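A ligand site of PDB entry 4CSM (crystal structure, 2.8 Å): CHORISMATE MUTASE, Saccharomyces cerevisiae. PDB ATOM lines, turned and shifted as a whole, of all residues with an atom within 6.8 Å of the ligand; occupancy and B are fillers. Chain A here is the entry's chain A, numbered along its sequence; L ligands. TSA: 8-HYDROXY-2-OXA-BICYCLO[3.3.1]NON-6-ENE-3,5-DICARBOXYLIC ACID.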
ATOM      1  N   LEU A  12       7.310  18.779   9.537  1.00  0.00           N
ATOM      2  CA  LEU A  12       6.728  17.857  10.512  1.00  0.00           C
ATOM      3  C   LEU A  12       7.718  17.065  11.378  1.00  0.00           C
ATOM      4  O   LEU A  12       7.570  16.975  12.606  1.00  0.00           O
ATOM      5  CB  LEU A  12       5.777  16.903   9.781  1.00  0.00           C
ATOM      6  CG  LEU A  12       4.917  16.003  10.663  1.00  0.00           C
ATOM      7  CD1 LEU A  12       4.140  16.839  11.665  1.00  0.00           C
ATOM      8  CD2 LEU A  12       3.970  15.201   9.787  1.00  0.00           C
ATOM      9  N   ILE A  15       9.247  19.505  13.816  1.00  0.00           N
ATOM     10  CA  ILE A  15       8.195  19.838  14.760  1.00  0.00           C
ATOM     11  C   ILE A  15       8.060  18.739  15.829  1.00  0.00           C
ATOM     12  O   ILE A  15       7.989  19.037  17.031  1.00  0.00           O
ATOM     13  CB  ILE A  15       6.870  20.023  14.016  1.00  0.00           C
ATOM     14  CG1 ILE A  15       7.046  21.073  12.910  1.00  0.00           C
ATOM     15  CG2 ILE A  15       5.798  20.489  14.973  1.00  0.00           C
ATOM     16  CD1 ILE A  15       5.816  21.292  12.068  1.00  0.00           C
ATOM     17  N   ARG A  16       8.053  17.486  15.396  1.00  0.00           N
ATOM     18  CA  ARG A  16       7.930  16.380  16.331  1.00  0.00           C
ATOM     19  C   ARG A  16       9.163  16.308  17.213  1.00  0.00           C
ATOM     20  O   ARG A  16       9.066  16.138  18.432  1.00  0.00           O
ATOM     21  CB  ARG A  16       7.741  15.060  15.587  1.00  0.00           C
ATOM     22  CG  ARG A  16       6.368  14.916  14.944  1.00  0.00           C
ATOM     23  CD  ARG A  16       6.184  13.561  14.249  1.00  0.00           C
ATOM     24  NE  ARG A  16       4.773  13.314  13.936  1.00  0.00           N
ATOM     25  CZ  ARG A  16       4.292  13.039  12.720  1.00  0.00           C
ATOM     26  NH1 ARG A  16       5.113  12.947  11.680  1.00  0.00           N
ATOM     27  NH2 ARG A  16       2.986  12.841  12.562  1.00  0.00           N
ATOM     28  N   LEU A  19       8.995  18.677  19.904  1.00  0.00           N
ATOM     29  CA  LEU A  19       8.023  18.179  20.874  1.00  0.00           C
ATOM     30  C   LEU A  19       8.675  17.164  21.807  1.00  0.00           C
ATOM     31  O   LEU A  19       8.395  17.136  23.022  1.00  0.00           O
ATOM     32  CB  LEU A  19       6.837  17.538  20.159  1.00  0.00           C
ATOM     33  CG  LEU A  19       5.949  18.577  19.473  1.00  0.00           C
ATOM     34  CD1 LEU A  19       4.917  17.923  18.606  1.00  0.00           C
ATOM     35  CD2 LEU A  19       5.296  19.440  20.528  1.00  0.00           C
ATOM     36  N   ARG A 157       3.933  23.621  24.042  1.00  0.00           N
ATOM     37  CA  ARG A 157       3.778  22.286  23.460  1.00  0.00           C
ATOM     38  C   ARG A 157       2.411  22.159  22.789  1.00  0.00           C
ATOM     39  O   ARG A 157       2.303  21.960  21.578  1.00  0.00           O
ATOM     40  CB  ARG A 157       3.881  21.252  24.582  1.00  0.00           C
ATOM     41  CG  ARG A 157       3.960  19.752  24.189  1.00  0.00           C
ATOM     42  CD  ARG A 157       2.823  19.234  23.305  1.00  0.00           C
ATOM     43  NE  ARG A 157       2.570  17.804  23.505  1.00  0.00           N
ATOM     44  CZ  ARG A 157       2.979  16.820  22.708  1.00  0.00           C
ATOM     45  NH1 ARG A 157       3.680  17.072  21.622  1.00  0.00           N
ATOM     46  NH2 ARG A 157       2.638  15.575  22.984  1.00  0.00           N
ATOM     47  N   GLY A 161       0.174  22.696  18.013  1.00  0.00           N
ATOM     48  CA  GLY A 161      -0.739  22.090  17.066  1.00  0.00           C
ATOM     49  C   GLY A 161      -0.885  22.887  15.789  1.00  0.00           C
ATOM     50  O   GLY A 161      -0.966  22.322  14.682  1.00  0.00           O
ATOM     51  N   VAL A 164       1.909  22.099  13.291  1.00  0.00           N
ATOM     52  CA  VAL A 164       1.689  20.747  12.805  1.00  0.00           C
ATOM     53  C   VAL A 164       0.574  20.816  11.795  1.00  0.00           C
ATOM     54  O   VAL A 164       0.724  20.355  10.642  1.00  0.00           O
ATOM     55  CB  VAL A 164       1.203  19.837  13.950  1.00  0.00           C
ATOM     56  CG1 VAL A 164       0.954  18.436  13.440  1.00  0.00           C
ATOM     57  CG2 VAL A 164       2.205  19.825  15.075  1.00  0.00           C
ATOM     58  N   LYS A 168       0.808  19.933   7.893  1.00  0.00           N
ATOM     59  CA  LYS A 168       0.029  18.859   7.291  1.00  0.00           C
ATOM     60  C   LYS A 168      -0.813  19.416   6.149  1.00  0.00           C
ATOM     61  O   LYS A 168      -0.845  18.862   5.045  1.00  0.00           O
ATOM     62  CB  LYS A 168      -0.895  18.213   8.346  1.00  0.00           C
ATOM     63  CG  LYS A 168      -0.166  17.478   9.458  1.00  0.00           C
ATOM     64  CD  LYS A 168      -1.109  16.883  10.484  1.00  0.00           C
ATOM     65  CE  LYS A 168      -0.306  16.170  11.586  1.00  0.00           C
ATOM     66  NZ  LYS A 168      -1.106  15.728  12.769  1.00  0.00           N
ATOM     67  N   MET A 189     -10.059  14.995  11.783  1.00  0.00           N
ATOM     68  CA  MET A 189      -9.506  14.344  12.969  1.00  0.00           C
ATOM     69  C   MET A 189      -8.780  13.028  12.659  1.00  0.00           C
ATOM     70  O   MET A 189      -7.579  12.903  12.874  1.00  0.00           O
ATOM     71  CB  MET A 189     -10.637  14.112  13.987  1.00  0.00           C
ATOM     72  CG  MET A 189     -10.241  13.405  15.293  1.00  0.00           C
ATOM     73  SD  MET A 189      -8.985  14.307  16.224  1.00  0.00           S
ATOM     74  CE  MET A 189      -9.846  15.984  16.518  1.00  0.00           C
ATOM     75  N   ILE A 192      -5.663  13.589  10.557  1.00  0.00           N
ATOM     76  CA  ILE A 192      -4.498  14.129  11.264  1.00  0.00           C
ATOM     77  C   ILE A 192      -3.962  13.186  12.356  1.00  0.00           C
ATOM     78  O   ILE A 192      -2.761  13.191  12.629  1.00  0.00           O
ATOM     79  CB  ILE A 192      -4.743  15.587  11.840  1.00  0.00           C
ATOM     80  CG1 ILE A 192      -5.893  15.682  12.855  1.00  0.00           C
ATOM     81  CG2 ILE A 192      -5.019  16.543  10.698  1.00  0.00           C
ATOM     82  CD1 ILE A 192      -5.629  15.174  14.260  1.00  0.00           C
ATOM     83  N   THR A 193      -4.833  12.368  12.935  1.00  0.00           N
ATOM     84  CA  THR A 193      -4.397  11.461  14.007  1.00  0.00           C
ATOM     85  C   THR A 193      -3.487  10.371  13.480  1.00  0.00           C
ATOM     86  O   THR A 193      -3.812   9.684  12.507  1.00  0.00           O
ATOM     87  CB  THR A 193      -5.608  10.767  14.750  1.00  0.00           C
ATOM     88  OG1 THR A 193      -6.476  11.762  15.337  1.00  0.00           O
ATOM     89  CG2 THR A 193      -5.093   9.801  15.844  1.00  0.00           C
ATOM     90  N   ASN A 194      -2.320  10.234  14.111  1.00  0.00           N
ATOM     91  CA  ASN A 194      -1.335   9.198  13.804  1.00  0.00           C
ATOM     92  C   ASN A 194      -1.036   8.459  15.126  1.00  0.00           C
ATOM     93  O   ASN A 194      -0.097   8.810  15.879  1.00  0.00           O
ATOM     94  CB  ASN A 194      -0.061   9.803  13.210  1.00  0.00           C
ATOM     95  CG  ASN A 194       1.018   8.761  12.967  1.00  0.00           C
ATOM     96  OD1 ASN A 194       1.256   7.870  13.799  1.00  0.00           O
ATOM     97  ND2 ASN A 194       1.696   8.888  11.828  1.00  0.00           N
ATOM     98  N   SER A 195      -1.815   7.412  15.386  1.00  0.00           N
ATOM     99  CA  SER A 195      -1.696   6.639  16.619  1.00  0.00           C
ATOM    100  C   SER A 195      -0.351   6.000  16.884  1.00  0.00           C
ATOM    101  O   SER A 195       0.007   5.763  18.046  1.00  0.00           O
ATOM    102  CB  SER A 195      -2.794   5.595  16.659  1.00  0.00           C
ATOM    103  OG  SER A 195      -4.044   6.240  16.541  1.00  0.00           O
ATOM    104  N   VAL A 197       2.700   7.317  16.180  1.00  0.00           N
ATOM    105  CA  VAL A 197       3.592   8.304  16.757  1.00  0.00           C
ATOM    106  C   VAL A 197       3.261   8.466  18.222  1.00  0.00           C
ATOM    107  O   VAL A 197       4.134   8.347  19.096  1.00  0.00           O
ATOM    108  CB  VAL A 197       3.429   9.683  16.089  1.00  0.00           C
ATOM    109  CG1 VAL A 197       4.140  10.742  16.912  1.00  0.00           C
ATOM    110  CG2 VAL A 197       4.029   9.657  14.715  1.00  0.00           C
ATOM    111  N   GLU A 198       1.988   8.755  18.466  1.00  0.00           N
ATOM    112  CA  GLU A 198       1.571   8.941  19.832  1.00  0.00           C
ATOM    113  C   GLU A 198       1.719   7.687  20.646  1.00  0.00           C
ATOM    114  O   GLU A 198       1.854   7.737  21.876  1.00  0.00           O
ATOM    115  CB  GLU A 198       0.190   9.606  19.944  1.00  0.00           C
ATOM    116  CG  GLU A 198      -0.892   9.187  18.982  1.00  0.00           C
ATOM    117  CD  GLU A 198      -2.165  10.036  19.206  1.00  0.00           C
ATOM    118  OE1 GLU A 198      -2.796   9.878  20.279  1.00  0.00           O
ATOM    119  OE2 GLU A 198      -2.511  10.873  18.322  1.00  0.00           O
ATOM    120  N   ILE A 201       5.446   7.890  21.935  1.00  0.00           N
ATOM    121  CA  ILE A 201       5.504   8.974  22.918  1.00  0.00           C
ATOM    122  C   ILE A 201       5.240   8.427  24.317  1.00  0.00           C
ATOM    123  O   ILE A 201       6.105   8.513  25.206  1.00  0.00           O
ATOM    124  CB  ILE A 201       4.462  10.043  22.614  1.00  0.00           C
ATOM    125  CG1 ILE A 201       4.747  10.713  21.277  1.00  0.00           C
ATOM    126  CG2 ILE A 201       4.405  11.063  23.758  1.00  0.00           C
ATOM    127  CD1 ILE A 201       3.737  11.797  20.930  1.00  0.00           C
ATOM    128  N   TYR A 234      -0.335  12.862  29.760  1.00  0.00           N
ATOM    129  CA  TYR A 234      -0.113  13.052  28.325  1.00  0.00           C
ATOM    130  C   TYR A 234      -1.255  12.443  27.479  1.00  0.00           C
ATOM    131  O   TYR A 234      -1.801  13.094  26.565  1.00  0.00           O
ATOM    132  CB  TYR A 234       1.249  12.475  27.908  1.00  0.00           C
ATOM    133  CG  TYR A 234       2.277  13.516  27.437  1.00  0.00           C
ATOM    134  CD1 TYR A 234       3.116  14.214  28.336  1.00  0.00           C
ATOM    135  CD2 TYR A 234       2.425  13.781  26.046  1.00  0.00           C
ATOM    136  CE1 TYR A 234       4.093  15.151  27.860  1.00  0.00           C
ATOM    137  CE2 TYR A 234       3.383  14.696  25.562  1.00  0.00           C
ATOM    138  CZ  TYR A 234       4.224  15.395  26.452  1.00  0.00           C
ATOM    139  OH  TYR A 234       5.155  16.286  25.907  1.00  0.00           O
ATOM    140  N   VAL A 238      -2.600  16.257  27.428  1.00  0.00           N
ATOM    141  CA  VAL A 238      -1.659  16.804  26.510  1.00  0.00           C
ATOM    142  C   VAL A 238      -1.908  16.456  25.049  1.00  0.00           C
ATOM    143  O   VAL A 238      -2.043  17.342  24.211  1.00  0.00           O
ATOM    144  CB  VAL A 238      -0.233  16.414  26.920  1.00  0.00           C
ATOM    145  CG1 VAL A 238       0.771  17.142  26.029  1.00  0.00           C
ATOM    146  CG2 VAL A 238      -0.026  16.719  28.417  1.00  0.00           C
ATOM    147  N   ILE A 239      -2.040  15.170  24.748  1.00  0.00           N
ATOM    148  CA  ILE A 239      -2.260  14.744  23.367  1.00  0.00           C
ATOM    149  C   ILE A 239      -3.647  15.116  22.829  1.00  0.00           C
ATOM    150  O   ILE A 239      -3.786  15.510  21.656  1.00  0.00           O
ATOM    151  CB  ILE A 239      -2.037  13.240  23.193  1.00  0.00           C
ATOM    152  CG1 ILE A 239      -0.643  12.858  23.701  1.00  0.00           C
ATOM    153  CG2 ILE A 239      -2.140  12.872  21.703  1.00  0.00           C
ATOM    154  CD1 ILE A 239      -0.358  11.403  23.590  1.00  0.00           C
ATOM    155  N   PRO A 240      -4.687  14.947  23.670  1.00  0.00           N
ATOM    156  CA  PRO A 240      -6.047  15.273  23.246  1.00  0.00           C
ATOM    157  C   PRO A 240      -6.154  16.728  22.778  1.00  0.00           C
ATOM    158  O   PRO A 240      -6.415  17.013  21.593  1.00  0.00           O
ATOM    159  CB  PRO A 240      -6.833  15.062  24.546  1.00  0.00           C
ATOM    160  CG  PRO A 240      -6.173  13.834  25.080  1.00  0.00           C
ATOM    161  CD  PRO A 240      -4.723  14.300  24.996  1.00  0.00           C
ATOM    162  N   THR A 242      -3.911  18.959  22.136  1.00  0.00           N
ATOM    163  CA  THR A 242      -3.061  19.377  21.024  1.00  0.00           C
ATOM    164  C   THR A 242      -3.871  19.160  19.738  1.00  0.00           C
ATOM    165  O   THR A 242      -3.881  20.027  18.843  1.00  0.00           O
ATOM    166  CB  THR A 242      -1.786  18.553  20.969  1.00  0.00           C
ATOM    167  OG1 THR A 242      -1.125  18.630  22.243  1.00  0.00           O
ATOM    168  CG2 THR A 242      -0.881  19.128  19.890  1.00  0.00           C
ATOM    169  N   LYS A 243      -4.587  18.033  19.671  1.00  0.00           N
ATOM    170  CA  LYS A 243      -5.426  17.756  18.516  1.00  0.00           C
ATOM    171  C   LYS A 243      -6.587  18.726  18.368  1.00  0.00           C
ATOM    172  O   LYS A 243      -6.882  19.131  17.232  1.00  0.00           O
ATOM    173  CB  LYS A 243      -5.848  16.293  18.434  1.00  0.00           C
ATOM    174  CG  LYS A 243      -4.703  15.423  17.908  1.00  0.00           C
ATOM    175  CD  LYS A 243      -5.022  13.936  17.795  1.00  0.00           C
ATOM    176  CE  LYS A 243      -5.244  13.292  19.140  1.00  0.00           C
ATOM    177  NZ  LYS A 243      -5.356  11.814  19.046  1.00  0.00           N
ATOM    178  N   GLU A 246      -5.302  21.561  16.657  1.00  0.00           N
ATOM    179  CA  GLU A 246      -5.100  21.158  15.274  1.00  0.00           C
ATOM    180  C   GLU A 246      -6.340  21.330  14.393  1.00  0.00           C
ATOM    181  O   GLU A 246      -6.262  21.968  13.314  1.00  0.00           O
ATOM    182  CB  GLU A 246      -4.573  19.741  15.205  1.00  0.00           C
ATOM    183  CG  GLU A 246      -3.209  19.589  15.869  1.00  0.00           C
ATOM    184  CD  GLU A 246      -2.595  18.229  15.610  1.00  0.00           C
ATOM    185  OE1 GLU A 246      -2.118  17.990  14.459  1.00  0.00           O
ATOM    186  OE2 GLU A 246      -2.588  17.393  16.539  1.00  0.00           O
HETATM  187  C1  TSA L   1       0.386  14.613  18.382  1.00  0.00           C
HETATM  188  C2  TSA L   1       0.884  13.256  17.878  1.00  0.00           C
HETATM  189  C3  TSA L   1       0.171  12.519  16.983  1.00  0.00           C
HETATM  190  C4  TSA L   1      -0.974  13.079  16.154  1.00  0.00           C
HETATM  191  O5  TSA L   1      -2.044  12.163  16.228  1.00  0.00           O
HETATM  192  C5  TSA L   1      -1.362  14.495  16.608  1.00  0.00           C
HETATM  193  C6  TSA L   1      -1.129  14.742  18.134  1.00  0.00           C
HETATM  194  O7  TSA L   1      -0.693  15.485  15.859  1.00  0.00           O
HETATM  195  C8  TSA L   1       0.685  15.768  16.148  1.00  0.00           C
HETATM  196  C9  TSA L   1       1.022  15.765  17.635  1.00  0.00           C
HETATM  197  C10 TSA L   1       0.847  14.775  19.827  1.00  0.00           C
HETATM  198  O1  TSA L   1       2.077  14.575  20.039  1.00  0.00           O
HETATM  199  O2  TSA L   1       0.017  15.093  20.698  1.00  0.00           O
HETATM  200  C11 TSA L   1       1.591  14.831  15.329  1.00  0.00           C
HETATM  201  O3  TSA L   1       2.713  14.540  15.763  1.00  0.00           O
HETATM  202  O4  TSA L   1       1.150  14.394  14.257  1.00  0.00           O
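OE2 of Glu 198 lies within hydrogen-bond range of O5 of the ligand (2.5 Å).
O5 of the ligand is in hydrogen-bond range of N of Asn 194, 2.9 Å away.
The guanidinium group (NH2) of Arg 16 lies within salt-bridge range of an oxygen (O4) of the ligand, at 2.9 Å.
O4 of the ligand is in salt-bridge range of NZ of Lys 168 (3.0 Å).
The guanidinium group (NH2) of Arg 157 is in salt-bridge range of an oxygen (O1) of the ligand (3.2 Å).
The side-chain amino group of Lys 243 lies within salt-bridge range of the side-chain carboxylate of Glu 198, at 3.1 Å.
NZ of Lys 168 is in salt-bridge range of OE1 of Glu 246 (3.0 Å).
The backbone NH (N) of Val 197 sits at hydrogen-bond distance from the side-chain amide oxygen (OD1) of Asn 194, 2.8 Å away.
The backbone carbonyl oxygen of Ile 192 is in hydrogen-bond range of the side-chain amino group of Lys 168 (3.0 Å).
The backbone carbonyl oxygen (O) of Tyr 234 lies within hydrogen-bond range of the backbone NH (N) of Ile 239 (2.8 Å).
The side-chain hydroxyl of Thr 193 is in hydrogen-bond range of the backbone carbonyl oxygen of Met 189 (2.9 Å).
The backbone carbonyl oxygen (O) of Val 238 is in hydrogen-bond range of the side-chain hydroxyl (OG1) of Thr 242 (2.5 Å).
OE2 of Glu 246 sits close to O7 of the ligand (2.8 Å).
Val 164 touches the ligand (CG1 to C8, 3.8 Å).
Ile 192 touches the ligand (O to O5, 3.8 Å).
Thr 193 touches the ligand (CA to O5, 3.3 Å).
Ile 201 touches the ligand (CD1 to O1, 3.4 Å).
Ile 239 touches the ligand.
CB of Thr 242 touches O2 of the ligand, at 3.9 Å.
CG of Lys 243 touches C6 of the ligand (3.6 Å).
Of the 23 residues printed, 13 come within 4 Å of the ligand.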
